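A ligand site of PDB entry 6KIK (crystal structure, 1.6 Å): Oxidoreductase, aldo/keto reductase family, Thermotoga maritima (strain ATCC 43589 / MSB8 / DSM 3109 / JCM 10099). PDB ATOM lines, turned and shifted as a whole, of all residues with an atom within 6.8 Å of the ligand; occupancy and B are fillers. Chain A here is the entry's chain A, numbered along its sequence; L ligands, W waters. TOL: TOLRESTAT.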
ATOM      1  N   TRP A  22     -22.001  -0.104 -32.883  1.00  0.00           N
ATOM      2  CA  TRP A  22     -23.441  -0.217 -33.056  1.00  0.00           C
ATOM      3  C   TRP A  22     -23.875   0.490 -34.333  1.00  0.00           C
ATOM      4  O   TRP A  22     -23.594   1.681 -34.529  1.00  0.00           O
ATOM      5  CB  TRP A  22     -24.133   0.390 -31.830  1.00  0.00           C
ATOM      6  CG  TRP A  22     -25.635   0.437 -31.860  1.00  0.00           C
ATOM      7  CD1 TRP A  22     -26.405   1.559 -31.807  1.00  0.00           C
ATOM      8  CD2 TRP A  22     -26.538  -0.673 -31.854  1.00  0.00           C
ATOM      9  NE1 TRP A  22     -27.740   1.217 -31.796  1.00  0.00           N
ATOM     10  CE2 TRP A  22     -27.848  -0.142 -31.823  1.00  0.00           C
ATOM     11  CE3 TRP A  22     -26.365  -2.062 -31.875  1.00  0.00           C
ATOM     12  CZ2 TRP A  22     -28.974  -0.960 -31.802  1.00  0.00           C
ATOM     13  CZ3 TRP A  22     -27.483  -2.869 -31.857  1.00  0.00           C
ATOM     14  CH2 TRP A  22     -28.791  -2.313 -31.830  1.00  0.00           C
ATOM     15  N   PHE A  27     -28.293  -2.685 -37.076  1.00  0.00           N
ATOM     16  CA  PHE A  27     -28.548  -2.425 -35.668  1.00  0.00           C
ATOM     17  C   PHE A  27     -29.071  -3.687 -35.002  1.00  0.00           C
ATOM     18  O   PHE A  27     -28.280  -4.527 -34.568  1.00  0.00           O
ATOM     19  CB  PHE A  27     -29.517  -1.244 -35.535  1.00  0.00           C
ATOM     20  CG  PHE A  27     -28.911   0.072 -35.926  1.00  0.00           C
ATOM     21  CD1 PHE A  27     -28.308   0.884 -34.984  1.00  0.00           C
ATOM     22  CD2 PHE A  27     -28.910   0.482 -37.248  1.00  0.00           C
ATOM     23  CE1 PHE A  27     -27.741   2.077 -35.339  1.00  0.00           C
ATOM     24  CE2 PHE A  27     -28.335   1.682 -37.622  1.00  0.00           C
ATOM     25  CZ  PHE A  27     -27.761   2.482 -36.671  1.00  0.00           C
ATOM     26  N   GLU A  28     -30.410  -3.863 -35.133  1.00  0.00           N
ATOM     27  CA  GLU A  28     -30.932  -5.090 -34.545  1.00  0.00           C
ATOM     28  C   GLU A  28     -30.871  -6.273 -35.492  1.00  0.00           C
ATOM     29  O   GLU A  28     -30.907  -7.421 -35.032  1.00  0.00           O
ATOM     30  CB  GLU A  28     -32.384  -4.851 -34.089  1.00  0.00           C
ATOM     31  CG  GLU A  28     -32.563  -3.617 -33.205  1.00  0.00           C
ATOM     32  CD  GLU A  28     -33.060  -2.393 -33.958  1.00  0.00           C
ATOM     33  OE1 GLU A  28     -32.771  -2.230 -35.163  1.00  0.00           O
ATOM     34  OE2 GLU A  28     -33.777  -1.567 -33.347  1.00  0.00           O
ATOM     35  N   ASP A  54     -15.379  -2.273 -29.530  1.00  0.00           N
ATOM     36  CA  ASP A  54     -16.497  -2.657 -28.679  1.00  0.00           C
ATOM     37  C   ASP A  54     -17.646  -3.136 -29.561  1.00  0.00           C
ATOM     38  O   ASP A  54     -18.116  -2.394 -30.425  1.00  0.00           O
ATOM     39  CB  ASP A  54     -16.943  -1.467 -27.812  1.00  0.00           C
ATOM     40  CG  ASP A  54     -18.063  -1.817 -26.844  1.00  0.00           C
ATOM     41  OD1 ASP A  54     -19.253  -1.669 -27.228  1.00  0.00           O
ATOM     42  OD2 ASP A  54     -17.770  -2.208 -25.696  1.00  0.00           O
ATOM     43  N   THR A  55     -18.079  -4.374 -29.350  1.00  0.00           N
ATOM     44  CA  THR A  55     -19.162  -4.941 -30.147  1.00  0.00           C
ATOM     45  C   THR A  55     -19.971  -5.878 -29.266  1.00  0.00           C
ATOM     46  O   THR A  55     -19.788  -5.914 -28.050  1.00  0.00           O
ATOM     47  CB  THR A  55     -18.596  -5.607 -31.410  1.00  0.00           C
ATOM     48  OG1 THR A  55     -19.642  -5.862 -32.344  1.00  0.00           O
ATOM     49  CG2 THR A  55     -17.897  -6.916 -31.091  1.00  0.00           C
ATOM     50  N   ALA A  56     -20.887  -6.627 -29.872  1.00  0.00           N
ATOM     51  CA  ALA A  56     -21.682  -7.593 -29.121  1.00  0.00           C
ATOM     52  C   ALA A  56     -22.301  -8.592 -30.087  1.00  0.00           C
ATOM     53  O   ALA A  56     -22.407  -8.317 -31.285  1.00  0.00           O
ATOM     54  CB  ALA A  56     -22.767  -6.903 -28.305  1.00  0.00           C
ATOM     55  N   TYR A  58     -25.313  -9.320 -30.541  1.00  0.00           N
ATOM     56  CA  TYR A  58     -26.582  -8.886 -31.122  1.00  0.00           C
ATOM     57  C   TYR A  58     -26.439  -7.679 -32.021  1.00  0.00           C
ATOM     58  O   TYR A  58     -27.424  -7.236 -32.610  1.00  0.00           O
ATOM     59  CB  TYR A  58     -27.594  -8.587 -30.003  1.00  0.00           C
ATOM     60  CG  TYR A  58     -26.993  -7.758 -28.905  1.00  0.00           C
ATOM     61  CD1 TYR A  58     -27.005  -6.371 -28.984  1.00  0.00           C
ATOM     62  CD2 TYR A  58     -26.371  -8.359 -27.826  1.00  0.00           C
ATOM     63  CE1 TYR A  58     -26.425  -5.593 -27.988  1.00  0.00           C
ATOM     64  CE2 TYR A  58     -25.779  -7.615 -26.830  1.00  0.00           C
ATOM     65  CZ  TYR A  58     -25.799  -6.225 -26.916  1.00  0.00           C
ATOM     66  OH  TYR A  58     -25.193  -5.482 -25.920  1.00  0.00           O
ATOM     67  N   TYR A  59     -25.229  -7.110 -32.116  1.00  0.00           N
ATOM     68  CA  TYR A  59     -24.993  -5.987 -33.021  1.00  0.00           C
ATOM     69  C   TYR A  59     -25.168  -6.459 -34.454  1.00  0.00           C
ATOM     70  O   TYR A  59     -24.491  -7.395 -34.890  1.00  0.00           O
ATOM     71  CB  TYR A  59     -23.573  -5.451 -32.825  1.00  0.00           C
ATOM     72  CG  TYR A  59     -23.351  -4.510 -31.673  1.00  0.00           C
ATOM     73  CD1 TYR A  59     -24.176  -4.517 -30.552  1.00  0.00           C
ATOM     74  CD2 TYR A  59     -22.289  -3.605 -31.702  1.00  0.00           C
ATOM     75  CE1 TYR A  59     -23.949  -3.660 -29.485  1.00  0.00           C
ATOM     76  CE2 TYR A  59     -22.048  -2.746 -30.665  1.00  0.00           C
ATOM     77  CZ  TYR A  59     -22.875  -2.770 -29.552  1.00  0.00           C
ATOM     78  OH  TYR A  59     -22.627  -1.909 -28.523  1.00  0.00           O
ATOM     79  N   LYS A  85     -20.107  -8.958 -25.936  1.00  0.00           N
ATOM     80  CA  LYS A  85     -21.111  -8.968 -24.889  1.00  0.00           C
ATOM     81  C   LYS A  85     -22.153 -10.037 -25.184  1.00  0.00           C
ATOM     82  O   LYS A  85     -22.377 -10.423 -26.337  1.00  0.00           O
ATOM     83  CB  LYS A  85     -21.817  -7.618 -24.745  1.00  0.00           C
ATOM     84  CG  LYS A  85     -20.902  -6.414 -24.887  1.00  0.00           C
ATOM     85  CD  LYS A  85     -21.646  -5.138 -24.599  1.00  0.00           C
ATOM     86  CE  LYS A  85     -20.749  -3.951 -24.843  1.00  0.00           C
ATOM     87  NZ  LYS A  85     -20.981  -3.361 -26.170  1.00  0.00           N
ATOM     88  N   TRP A  87     -26.243 -11.151 -24.625  1.00  0.00           N
ATOM     89  CA  TRP A  87     -27.585 -10.633 -24.390  1.00  0.00           C
ATOM     90  C   TRP A  87     -28.203 -11.334 -23.172  1.00  0.00           C
ATOM     91  O   TRP A  87     -27.897 -12.491 -22.906  1.00  0.00           O
ATOM     92  CB  TRP A  87     -28.426 -10.889 -25.648  1.00  0.00           C
ATOM     93  CG  TRP A  87     -29.808 -10.280 -25.652  1.00  0.00           C
ATOM     94  CD1 TRP A  87     -30.991 -10.956 -25.520  1.00  0.00           C
ATOM     95  CD2 TRP A  87     -30.150  -8.900 -25.817  1.00  0.00           C
ATOM     96  NE1 TRP A  87     -32.061 -10.077 -25.575  1.00  0.00           N
ATOM     97  CE2 TRP A  87     -31.560  -8.808 -25.747  1.00  0.00           C
ATOM     98  CE3 TRP A  87     -29.404  -7.742 -25.990  1.00  0.00           C
ATOM     99  CZ2 TRP A  87     -32.241  -7.584 -25.864  1.00  0.00           C
ATOM    100  CZ3 TRP A  87     -30.083  -6.509 -26.102  1.00  0.00           C
ATOM    101  CH2 TRP A  87     -31.490  -6.456 -26.044  1.00  0.00           C
ATOM    102  N   LEU A 116     -18.567  -9.140 -21.640  1.00  0.00           N
ATOM    103  CA  LEU A 116     -19.473  -8.461 -20.695  1.00  0.00           C
ATOM    104  C   LEU A 116     -20.887  -9.053 -20.722  1.00  0.00           C
ATOM    105  O   LEU A 116     -21.334  -9.428 -21.733  1.00  0.00           O
ATOM    106  CB  LEU A 116     -19.650  -6.995 -21.105  1.00  0.00           C
ATOM    107  CG  LEU A 116     -18.399  -6.149 -21.329  1.00  0.00           C
ATOM    108  CD1 LEU A 116     -18.800  -4.743 -21.685  1.00  0.00           C
ATOM    109  CD2 LEU A 116     -17.528  -6.107 -20.115  1.00  0.00           C
ATOM    110  N   HIS A 118     -24.407  -7.958 -20.999  1.00  0.00           N
ATOM    111  CA  HIS A 118     -24.959  -6.691 -21.522  1.00  0.00           C
ATOM    112  C   HIS A 118     -25.945  -6.047 -20.556  1.00  0.00           C
ATOM    113  O   HIS A 118     -25.956  -4.859 -20.446  1.00  0.00           O
ATOM    114  CB  HIS A 118     -25.685  -6.919 -22.844  1.00  0.00           C
ATOM    115  CG  HIS A 118     -26.572  -5.786 -23.246  1.00  0.00           C
ATOM    116  ND1 HIS A 118     -26.122  -4.519 -23.428  1.00  0.00           N
ATOM    117  CD2 HIS A 118     -27.895  -5.741 -23.524  1.00  0.00           C
ATOM    118  CE1 HIS A 118     -27.122  -3.748 -23.765  1.00  0.00           C
ATOM    119  NE2 HIS A 118     -28.206  -4.456 -23.825  1.00  0.00           N
ATOM    120  N   TRP A 119     -26.765  -6.867 -19.901  1.00  0.00           N
ATOM    121  CA  TRP A 119     -27.835  -6.327 -19.076  1.00  0.00           C
ATOM    122  C   TRP A 119     -28.184  -7.400 -18.065  1.00  0.00           C
ATOM    123  O   TRP A 119     -28.208  -8.582 -18.421  1.00  0.00           O
ATOM    124  CB  TRP A 119     -29.074  -5.962 -19.922  1.00  0.00           C
ATOM    125  CG  TRP A 119     -30.024  -4.961 -19.258  1.00  0.00           C
ATOM    126  CD1 TRP A 119     -31.011  -5.231 -18.345  1.00  0.00           C
ATOM    127  CD2 TRP A 119     -30.074  -3.549 -19.505  1.00  0.00           C
ATOM    128  NE1 TRP A 119     -31.655  -4.057 -18.001  1.00  0.00           N
ATOM    129  CE2 TRP A 119     -31.095  -3.019 -18.692  1.00  0.00           C
ATOM    130  CE3 TRP A 119     -29.346  -2.681 -20.317  1.00  0.00           C
ATOM    131  CZ2 TRP A 119     -31.404  -1.649 -18.674  1.00  0.00           C
ATOM    132  CZ3 TRP A 119     -29.657  -1.329 -20.307  1.00  0.00           C
ATOM    133  CH2 TRP A 119     -30.673  -0.826 -19.484  1.00  0.00           C
ATOM    134  N   SER A 148     -22.122  -4.815 -17.694  1.00  0.00           N
ATOM    135  CA  SER A 148     -22.647  -3.624 -18.322  1.00  0.00           C
ATOM    136  C   SER A 148     -24.030  -3.354 -17.781  1.00  0.00           C
ATOM    137  O   SER A 148     -24.807  -4.288 -17.560  1.00  0.00           O
ATOM    138  CB  SER A 148     -22.677  -3.780 -19.849  1.00  0.00           C
ATOM    139  OG  SER A 148     -23.087  -2.574 -20.484  1.00  0.00           O
ATOM    140  N   ASN A 149     -24.335  -2.079 -17.534  1.00  0.00           N
ATOM    141  CA  ASN A 149     -25.650  -1.651 -17.061  1.00  0.00           C
ATOM    142  C   ASN A 149     -25.975  -2.276 -15.710  1.00  0.00           C
ATOM    143  O   ASN A 149     -27.136  -2.574 -15.420  1.00  0.00           O
ATOM    144  CB  ASN A 149     -26.719  -1.975 -18.104  1.00  0.00           C
ATOM    145  CG  ASN A 149     -26.449  -1.263 -19.392  1.00  0.00           C
ATOM    146  OD1 ASN A 149     -26.437  -0.024 -19.421  1.00  0.00           O
ATOM    147  ND2 ASN A 149     -26.162  -2.006 -20.453  1.00  0.00           N
ATOM    148  N   GLN A 170     -19.688  -1.175 -17.824  1.00  0.00           N
ATOM    149  CA  GLN A 170     -19.988  -0.290 -18.939  1.00  0.00           C
ATOM    150  C   GLN A 170     -21.408   0.249 -18.782  1.00  0.00           C
ATOM    151  O   GLN A 170     -22.384  -0.526 -18.840  1.00  0.00           O
ATOM    152  CB  GLN A 170     -19.820  -1.017 -20.275  1.00  0.00           C
ATOM    153  CG  GLN A 170     -20.143  -0.121 -21.456  1.00  0.00           C
ATOM    154  CD  GLN A 170     -19.840  -0.766 -22.783  1.00  0.00           C
ATOM    155  OE1 GLN A 170     -18.783  -1.383 -22.982  1.00  0.00           O
ATOM    156  NE2 GLN A 170     -20.752  -0.623 -23.718  1.00  0.00           N
ATOM    157  N   TYR A 199     -20.726   4.567 -22.034  1.00  0.00           N
ATOM    158  CA  TYR A 199     -21.281   4.536 -23.386  1.00  0.00           C
ATOM    159  C   TYR A 199     -22.275   5.671 -23.556  1.00  0.00           C
ATOM    160  O   TYR A 199     -22.692   6.333 -22.604  1.00  0.00           O
ATOM    161  CB  TYR A 199     -21.894   3.168 -23.720  1.00  0.00           C
ATOM    162  CG  TYR A 199     -23.202   2.801 -23.082  1.00  0.00           C
ATOM    163  CD1 TYR A 199     -24.411   3.187 -23.645  1.00  0.00           C
ATOM    164  CD2 TYR A 199     -23.235   1.986 -21.955  1.00  0.00           C
ATOM    165  CE1 TYR A 199     -25.621   2.808 -23.074  1.00  0.00           C
ATOM    166  CE2 TYR A 199     -24.446   1.607 -21.384  1.00  0.00           C
ATOM    167  CZ  TYR A 199     -25.625   2.009 -21.939  1.00  0.00           C
ATOM    168  OH  TYR A 199     -26.814   1.634 -21.357  1.00  0.00           O
ATOM    169  N   SER A 200     -22.635   5.900 -24.817  1.00  0.00           N
ATOM    170  CA  SER A 200     -23.284   7.149 -25.210  1.00  0.00           C
ATOM    171  C   SER A 200     -22.579   8.340 -24.583  1.00  0.00           C
ATOM    172  O   SER A 200     -23.229   9.206 -23.976  1.00  0.00           O
ATOM    173  CB  SER A 200     -24.761   7.117 -24.833  1.00  0.00           C
ATOM    174  OG  SER A 200     -25.399   6.080 -25.544  1.00  0.00           O
ATOM    175  N   LYS A 245     -19.751   6.299 -30.407  1.00  0.00           N
ATOM    176  CA  LYS A 245     -20.151   5.618 -31.629  1.00  0.00           C
ATOM    177  C   LYS A 245     -19.274   6.089 -32.785  1.00  0.00           C
ATOM    178  O   LYS A 245     -19.121   7.296 -32.991  1.00  0.00           O
ATOM    179  CB  LYS A 245     -21.636   5.855 -31.906  1.00  0.00           C
ATOM    180  CG  LYS A 245     -22.331   4.764 -32.728  1.00  0.00           C
ATOM    181  CD  LYS A 245     -22.047   3.345 -32.202  1.00  0.00           C
ATOM    182  CE  LYS A 245     -22.221   3.193 -30.686  1.00  0.00           C
ATOM    183  NZ  LYS A 245     -21.531   1.976 -30.177  1.00  0.00           N
HETATM  184  C1  TOL L   1     -32.877  -1.989 -29.645  1.00  0.00           C
HETATM  185  F1  TOL L   1     -33.408  -3.166 -29.882  1.00  0.00           F
HETATM  186  F2  TOL L   1     -33.684  -1.380 -28.785  1.00  0.00           F
HETATM  187  F3  TOL L   1     -32.738  -1.286 -30.744  1.00  0.00           F
HETATM  188  C2  TOL L   1     -31.533  -2.153 -28.993  1.00  0.00           C
HETATM  189  C3  TOL L   1     -30.856  -3.469 -28.989  1.00  0.00           C
HETATM  190  O1  TOL L   1     -31.478  -4.521 -29.598  1.00  0.00           O
HETATM  191  C4  TOL L   1     -30.742  -5.715 -29.895  1.00  0.00           C
HETATM  192  C5  TOL L   1     -29.603  -3.604 -28.380  1.00  0.00           C
HETATM  193  C6  TOL L   1     -28.950  -2.527 -27.759  1.00  0.00           C
HETATM  194  C7  TOL L   1     -29.531  -1.265 -27.740  1.00  0.00           C
HETATM  195  C8  TOL L   1     -28.863  -0.098 -27.101  1.00  0.00           C
HETATM  196  C9  TOL L   1     -29.482   1.143 -27.099  1.00  0.00           C
HETATM  197  C10 TOL L   1     -30.732   1.315 -27.692  1.00  0.00           C
HETATM  198  C11 TOL L   1     -31.404   0.267 -28.323  1.00  0.00           C
HETATM  199  C12 TOL L   1     -30.852  -1.012 -28.350  1.00  0.00           C
HETATM  200  C13 TOL L   1     -27.539  -0.254 -26.438  1.00  0.00           C
HETATM  201  S1  TOL L   1     -27.555  -0.225 -24.868  1.00  0.00           S
HETATM  202  N1  TOL L   1     -26.420  -0.416 -27.135  1.00  0.00           N
HETATM  203  C14 TOL L   1     -26.398  -0.479 -28.587  1.00  0.00           C
HETATM  204  C15 TOL L   1     -25.103  -0.545 -26.530  1.00  0.00           C
HETATM  205  C16 TOL L   1     -24.797  -1.981 -26.165  1.00  0.00           C
HETATM  206  O2  TOL L   1     -23.722  -2.210 -25.555  1.00  0.00           O
HETATM  207  O3  TOL L   1     -25.604  -2.881 -26.466  1.00  0.00           O
HETATM  208  O   HOH W   1     -25.350  -0.786 -23.079  1.00  0.00           O
HETATM  209  O   HOH W   2     -23.718  -3.416 -23.012  1.00  0.00           O
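A fluorine (F3) of the ligand sits close to the side-chain carboxylate (OE2) of Glu 28 (2.8 Å).
CD2 of Trp 22 touches C14 of the ligand (3.3 Å).
CZ3 of Trp 87 touches C5 of the ligand, at 3.7 Å.
Gln 170 touches the ligand.
Along chain A the residues within 4 Å of the ligand span positions 22 to 170.
OH of Tyr 58 lies within hydrogen-bond range of O3 of the ligand (2.7 Å).
NZ of Lys 85 is in salt-bridge range of O2 of the ligand (3.0 Å).
OH of Tyr 59 lies within hydrogen-bond range of O2 of the ligand (3.2 Å).
ND1 of His 118 sits close to O3 of the ligand, at 3.5 Å.
The side-chain hydroxyl of Tyr 58 sits at hydrogen-bond distance from a ring nitrogen (ND1) of His 118 (2.8 Å).
NZ of Lys 85 lies within hydrogen-bond range of OH of Tyr 59 (3.2 Å).
The side-chain amino group of Lys 85 lies within salt-bridge range of the side-chain carboxylate of Asp 54, at 2.6 Å.
The backbone carbonyl oxygen (O) of Thr 55 sits at hydrogen-bond distance from the side-chain amino group (NZ) of Lys 85.
The side-chain amide nitrogen of Asn 149 lies within hydrogen-bond range of the backbone carbonyl oxygen of His 118, at 2.9 Å.
OD2 of Asp 54 sits close to OE1 of Gln 170 (3.0 Å).
O of Gln 170 sits at hydrogen-bond distance from N of Asn 149 (2.8 Å).
The backbone carbonyl oxygen of Gln 170 is in hydrogen-bond range of the side-chain hydroxyl of Ser 148 (2.7 Å).
Water W2 lies within hydrogen-bond range of a ring nitrogen (ND1) of His 118 (2.7 Å), the side-chain hydroxyl of Ser 148 (2.7 Å) and an oxygen (O2) of the ligand (2.8 Å).
Water W1 lies within hydrogen-bond range of a sulfur (S1) of the ligand (2.9 Å), the side-chain amide nitrogen (ND2) of Asn 149 (3.0 Å) and the side-chain hydroxyl (OH) of Tyr 199 (3.3 Å).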
